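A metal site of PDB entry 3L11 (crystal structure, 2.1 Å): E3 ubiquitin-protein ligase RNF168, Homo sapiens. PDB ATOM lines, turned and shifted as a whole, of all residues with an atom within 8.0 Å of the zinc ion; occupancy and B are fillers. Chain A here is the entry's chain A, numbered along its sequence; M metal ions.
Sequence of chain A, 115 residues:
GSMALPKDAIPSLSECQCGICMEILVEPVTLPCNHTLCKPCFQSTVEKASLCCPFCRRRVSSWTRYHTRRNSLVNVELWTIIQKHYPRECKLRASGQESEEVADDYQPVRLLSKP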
ATOM      1  N   GLN A  17      28.455  25.023 -17.021  1.00  0.00           N
ATOM      2  CA  GLN A  17      29.372  24.662 -18.118  1.00  0.00           C
ATOM      3  C   GLN A  17      28.571  24.158 -19.328  1.00  0.00           C
ATOM      4  O   GLN A  17      27.550  23.506 -19.154  1.00  0.00           O
ATOM      5  CB  GLN A  17      30.318  23.557 -17.667  1.00  0.00           C
ATOM      6  CG  GLN A  17      31.436  24.056 -16.755  1.00  0.00           C
ATOM      7  CD  GLN A  17      32.255  22.901 -16.302  1.00  0.00           C
ATOM      8  OE1 GLN A  17      31.978  22.394 -15.236  1.00  0.00           O
ATOM      9  NE2 GLN A  17      33.213  22.421 -17.132  1.00  0.00           N
ATOM     10  N   CYS A  18      29.071  24.430 -20.544  1.00  0.00           N
ATOM     11  CA  CYS A  18      28.429  23.972 -21.713  1.00  0.00           C
ATOM     12  C   CYS A  18      28.680  22.454 -21.729  1.00  0.00           C
ATOM     13  O   CYS A  18      29.801  22.011 -21.563  1.00  0.00           O
ATOM     14  CB  CYS A  18      29.067  24.646 -22.874  1.00  0.00           C
ATOM     15  SG  CYS A  18      28.410  23.990 -24.414  1.00  0.00           S
ATOM     16  N   GLY A  19      27.643  21.645 -21.897  1.00  0.00           N
ATOM     17  CA  GLY A  19      27.807  20.163 -21.950  1.00  0.00           C
ATOM     18  C   GLY A  19      28.437  19.695 -23.243  1.00  0.00           C
ATOM     19  O   GLY A  19      28.726  18.527 -23.386  1.00  0.00           O
ATOM     20  N   ILE A  20      28.686  20.583 -24.190  1.00  0.00           N
ATOM     21  CA  ILE A  20      29.386  20.143 -25.352  1.00  0.00           C
ATOM     22  C   ILE A  20      30.886  20.375 -25.195  1.00  0.00           C
ATOM     23  O   ILE A  20      31.680  19.498 -25.455  1.00  0.00           O
ATOM     24  CB  ILE A  20      28.798  20.785 -26.628  1.00  0.00           C
ATOM     25  CG1 ILE A  20      27.390  20.232 -26.854  1.00  0.00           C
ATOM     26  CG2 ILE A  20      29.670  20.543 -27.908  1.00  0.00           C
ATOM     27  CD1 ILE A  20      26.737  21.166 -27.639  1.00  0.00           C
ATOM     28  N   CYS A  21      31.286  21.559 -24.784  1.00  0.00           N
ATOM     29  CA  CYS A  21      32.681  21.897 -24.919  1.00  0.00           C
ATOM     30  C   CYS A  21      33.279  21.985 -23.516  1.00  0.00           C
ATOM     31  O   CYS A  21      34.460  22.184 -23.425  1.00  0.00           O
ATOM     32  CB  CYS A  21      32.836  23.213 -25.694  1.00  0.00           C
ATOM     33  SG  CYS A  21      32.149  24.655 -24.719  1.00  0.00           S
ATOM     34  N   MET A  22      32.480  21.841 -22.453  1.00  0.00           N
ATOM     35  CA  MET A  22      32.917  21.981 -21.045  1.00  0.00           C
ATOM     36  C   MET A  22      33.406  23.363 -20.633  1.00  0.00           C
ATOM     37  O   MET A  22      33.856  23.504 -19.503  1.00  0.00           O
ATOM     38  CB  MET A  22      34.052  21.036 -20.622  1.00  0.00           C
ATOM     39  CG  MET A  22      33.809  19.524 -20.576  1.00  0.00           C
ATOM     40  SD  MET A  22      32.082  19.086 -20.575  1.00  0.00           S
ATOM     41  CE  MET A  22      31.312  19.531 -18.994  1.00  0.00           C
ATOM     42  N   GLU A  23      33.417  24.362 -21.497  1.00  0.00           N
ATOM     43  CA  GLU A  23      33.757  25.732 -21.052  1.00  0.00           C
ATOM     44  C   GLU A  23      32.524  26.294 -20.338  1.00  0.00           C
ATOM     45  O   GLU A  23      31.414  25.826 -20.586  1.00  0.00           O
ATOM     46  CB  GLU A  23      34.121  26.608 -22.245  1.00  0.00           C
ATOM     47  CG  GLU A  23      35.269  26.037 -23.094  1.00  0.00           C
ATOM     48  CD  GLU A  23      36.578  25.955 -22.300  1.00  0.00           C
ATOM     49  OE1 GLU A  23      36.813  26.741 -21.355  1.00  0.00           O
ATOM     50  OE2 GLU A  23      37.390  25.084 -22.591  1.00  0.00           O
ATOM     51  N   ILE A  24      32.714  27.290 -19.463  1.00  0.00           N
ATOM     52  CA  ILE A  24      31.581  28.100 -18.965  1.00  0.00           C
ATOM     53  C   ILE A  24      30.651  28.471 -20.169  1.00  0.00           C
ATOM     54  O   ILE A  24      31.099  28.799 -21.279  1.00  0.00           O
ATOM     55  CB  ILE A  24      32.062  29.384 -18.223  1.00  0.00           C
ATOM     56  CG1 ILE A  24      30.929  30.068 -17.462  1.00  0.00           C
ATOM     57  CG2 ILE A  24      32.643  30.426 -19.162  1.00  0.00           C
ATOM     58  CD1 ILE A  24      30.710  29.509 -16.082  1.00  0.00           C
ATOM     59  N   LEU A  25      29.342  28.386 -19.940  1.00  0.00           N
ATOM     60  CA  LEU A  25      28.352  28.718 -20.918  1.00  0.00           C
ATOM     61  C   LEU A  25      28.450  30.208 -21.246  1.00  0.00           C
ATOM     62  O   LEU A  25      28.343  31.050 -20.349  1.00  0.00           O
ATOM     63  CB  LEU A  25      27.023  28.416 -20.240  1.00  0.00           C
ATOM     64  CG  LEU A  25      25.919  27.495 -20.702  1.00  0.00           C
ATOM     65  CD1 LEU A  25      26.206  26.583 -21.917  1.00  0.00           C
ATOM     66  CD2 LEU A  25      25.187  26.808 -19.543  1.00  0.00           C
ATOM     67  N   VAL A  26      28.687  30.579 -22.493  1.00  0.00           N
ATOM     68  CA  VAL A  26      28.690  31.985 -22.885  1.00  0.00           C
ATOM     69  C   VAL A  26      27.494  32.192 -23.849  1.00  0.00           C
ATOM     70  O   VAL A  26      27.291  31.350 -24.737  1.00  0.00           O
ATOM     71  CB  VAL A  26      30.081  32.374 -23.468  1.00  0.00           C
ATOM     72  CG1 VAL A  26      29.979  33.637 -24.315  1.00  0.00           C
ATOM     73  CG2 VAL A  26      31.090  32.591 -22.276  1.00  0.00           C
ATOM     74  N   THR A  36      20.520  23.169 -23.300  1.00  0.00           N
ATOM     75  CA  THR A  36      21.266  24.385 -23.487  1.00  0.00           C
ATOM     76  C   THR A  36      22.699  24.106 -23.945  1.00  0.00           C
ATOM     77  O   THR A  36      23.291  23.092 -23.578  1.00  0.00           O
ATOM     78  CB  THR A  36      21.230  25.181 -22.187  1.00  0.00           C
ATOM     79  OG1 THR A  36      19.883  25.639 -22.040  1.00  0.00           O
ATOM     80  CG2 THR A  36      22.004  26.415 -22.309  1.00  0.00           C
ATOM     81  N   LEU A  37      23.209  24.983 -24.771  1.00  0.00           N
ATOM     82  CA  LEU A  37      24.630  24.928 -25.105  1.00  0.00           C
ATOM     83  C   LEU A  37      25.166  26.368 -25.378  1.00  0.00           C
ATOM     84  O   LEU A  37      24.368  27.317 -25.552  1.00  0.00           O
ATOM     85  CB  LEU A  37      24.852  23.974 -26.317  1.00  0.00           C
ATOM     86  CG  LEU A  37      24.486  24.532 -27.687  1.00  0.00           C
ATOM     87  CD1 LEU A  37      24.922  23.590 -28.789  1.00  0.00           C
ATOM     88  CD2 LEU A  37      22.931  24.643 -27.743  1.00  0.00           C
ATOM     89  N   CYS A  38      26.491  26.574 -25.367  1.00  0.00           N
ATOM     90  CA  CYS A  38      26.969  27.950 -25.498  1.00  0.00           C
ATOM     91  C   CYS A  38      26.726  28.373 -26.946  1.00  0.00           C
ATOM     92  O   CYS A  38      26.641  27.517 -27.843  1.00  0.00           O
ATOM     93  CB  CYS A  38      28.459  28.072 -25.129  1.00  0.00           C
ATOM     94  SG  CYS A  38      29.602  27.074 -26.188  1.00  0.00           S
ATOM     95  N   LYS A  39      26.664  29.682 -27.208  1.00  0.00           N
ATOM     96  CA  LYS A  39      26.445  30.148 -28.569  1.00  0.00           C
ATOM     97  C   LYS A  39      27.533  29.655 -29.550  1.00  0.00           C
ATOM     98  O   LYS A  39      27.175  29.139 -30.623  1.00  0.00           O
ATOM     99  CB  LYS A  39      26.286  31.677 -28.575  1.00  0.00           C
ATOM    100  CG  LYS A  39      26.191  32.301 -29.933  1.00  0.00           C
ATOM    101  CD  LYS A  39      24.824  32.818 -30.196  1.00  0.00           C
ATOM    102  CE  LYS A  39      25.023  34.332 -30.586  1.00  0.00           C
ATOM    103  NZ  LYS A  39      23.755  35.055 -31.056  1.00  0.00           N
ATOM    104  N   PRO A  40      28.841  29.779 -29.197  1.00  0.00           N
ATOM    105  CA  PRO A  40      29.797  29.127 -30.123  1.00  0.00           C
ATOM    106  C   PRO A  40      29.484  27.663 -30.455  1.00  0.00           C
ATOM    107  O   PRO A  40      29.550  27.261 -31.627  1.00  0.00           O
ATOM    108  CB  PRO A  40      31.138  29.253 -29.398  1.00  0.00           C
ATOM    109  CG  PRO A  40      31.001  30.558 -28.599  1.00  0.00           C
ATOM    110  CD  PRO A  40      29.535  30.556 -28.134  1.00  0.00           C
ATOM    111  N   CYS A  41      29.186  26.824 -29.472  1.00  0.00           N
ATOM    112  CA  CYS A  41      28.788  25.440 -29.789  1.00  0.00           C
ATOM    113  C   CYS A  41      27.527  25.330 -30.644  1.00  0.00           C
ATOM    114  O   CYS A  41      27.421  24.456 -31.528  1.00  0.00           O
ATOM    115  CB  CYS A  41      28.634  24.602 -28.539  1.00  0.00           C
ATOM    116  SG  CYS A  41      30.269  24.080 -27.909  1.00  0.00           S
ATOM    117  N   PHE A  42      26.555  26.183 -30.385  1.00  0.00           N
ATOM    118  CA  PHE A  42      25.342  26.172 -31.182  1.00  0.00           C
ATOM    119  C   PHE A  42      25.695  26.451 -32.632  1.00  0.00           C
ATOM    120  O   PHE A  42      25.129  25.845 -33.513  1.00  0.00           O
ATOM    121  CB  PHE A  42      24.370  27.233 -30.650  1.00  0.00           C
ATOM    122  CG  PHE A  42      23.197  27.442 -31.518  1.00  0.00           C
ATOM    123  CD1 PHE A  42      22.103  26.557 -31.466  1.00  0.00           C
ATOM    124  CD2 PHE A  42      23.143  28.521 -32.431  1.00  0.00           C
ATOM    125  CE1 PHE A  42      20.964  26.744 -32.281  1.00  0.00           C
ATOM    126  CE2 PHE A  42      21.952  28.713 -33.225  1.00  0.00           C
ATOM    127  CZ  PHE A  42      20.902  27.810 -33.154  1.00  0.00           C
ATOM    128  N   THR A  45      27.780  23.059 -33.820  1.00  0.00           N
ATOM    129  CA  THR A  45      27.239  21.725 -33.741  1.00  0.00           C
ATOM    130  C   THR A  45      25.803  21.752 -34.187  1.00  0.00           C
ATOM    131  O   THR A  45      25.203  20.680 -34.324  1.00  0.00           O
ATOM    132  CB  THR A  45      27.356  21.091 -32.306  1.00  0.00           C
ATOM    133  OG1 THR A  45      26.584  21.867 -31.392  1.00  0.00           O
ATOM    134  CG2 THR A  45      28.757  21.155 -31.839  1.00  0.00           C
ATOM    135  N   PHE A  55      21.802  17.055 -27.956  1.00  0.00           N
ATOM    136  CA  PHE A  55      21.471  16.178 -26.833  1.00  0.00           C
ATOM    137  C   PHE A  55      20.332  15.203 -27.101  1.00  0.00           C
ATOM    138  O   PHE A  55      20.402  14.083 -26.639  1.00  0.00           O
ATOM    139  CB  PHE A  55      21.204  16.944 -25.533  1.00  0.00           C
ATOM    140  CG  PHE A  55      22.313  17.885 -25.176  1.00  0.00           C
ATOM    141  CD1 PHE A  55      23.375  17.486 -24.387  1.00  0.00           C
ATOM    142  CD2 PHE A  55      22.278  19.216 -25.646  1.00  0.00           C
ATOM    143  CE1 PHE A  55      24.385  18.387 -24.057  1.00  0.00           C
ATOM    144  CE2 PHE A  55      23.314  20.122 -25.332  1.00  0.00           C
ATOM    145  CZ  PHE A  55      24.353  19.692 -24.511  1.00  0.00           C
ATOM    146  N   ARG A  93      36.625  33.614 -20.733  1.00  0.00           N
ATOM    147  CA  ARG A  93      36.258  32.956 -21.946  1.00  0.00           C
ATOM    148  C   ARG A  93      36.234  33.989 -23.041  1.00  0.00           C
ATOM    149  O   ARG A  93      36.830  33.741 -24.072  1.00  0.00           O
ATOM    150  CB  ARG A  93      34.929  32.258 -21.860  1.00  0.00           C
ATOM    151  CG  ARG A  93      34.809  31.349 -23.078  1.00  0.00           C
ATOM    152  CD  ARG A  93      33.779  30.341 -22.931  1.00  0.00           C
ATOM    153  NE  ARG A  93      33.634  29.822 -24.255  1.00  0.00           N
ATOM    154  CZ  ARG A  93      32.689  29.018 -24.714  1.00  0.00           C
ATOM    155  NH1 ARG A  93      31.684  28.562 -23.932  1.00  0.00           N
ATOM    156  NH2 ARG A  93      32.768  28.717 -25.994  1.00  0.00           N
HETATM  157 ZN    ZN M   1      30.039  24.976 -25.722  1.00  0.00          ZN
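The zinc ion is bound by SG of Cys 38, SG of Cys 18, SG of Cys 21 and SG of Cys 41.
The zinc ion has four donor atoms within binding distance.
The guanidinium group (NH1) of Arg 93 sits close to the side-chain sulfur (SG) of Cys 38 (3.4 Å).
The side-chain sulfur (SG) of Cys 18 lies close to the backbone NH (N) of Ile 20 (3.4 Å).
N of Cys 18 lies within hydrogen-bond range of O of Glu 23 (2.7 Å).
SG of Cys 21 lies close to N of Glu 23 (3.5 Å).
O of Cys 41 lies within hydrogen-bond range of OG1 of Thr 45 (2.7 Å).
The nearest printed residue that does not touch the zinc ion is Arg 93 (4.3 Å).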
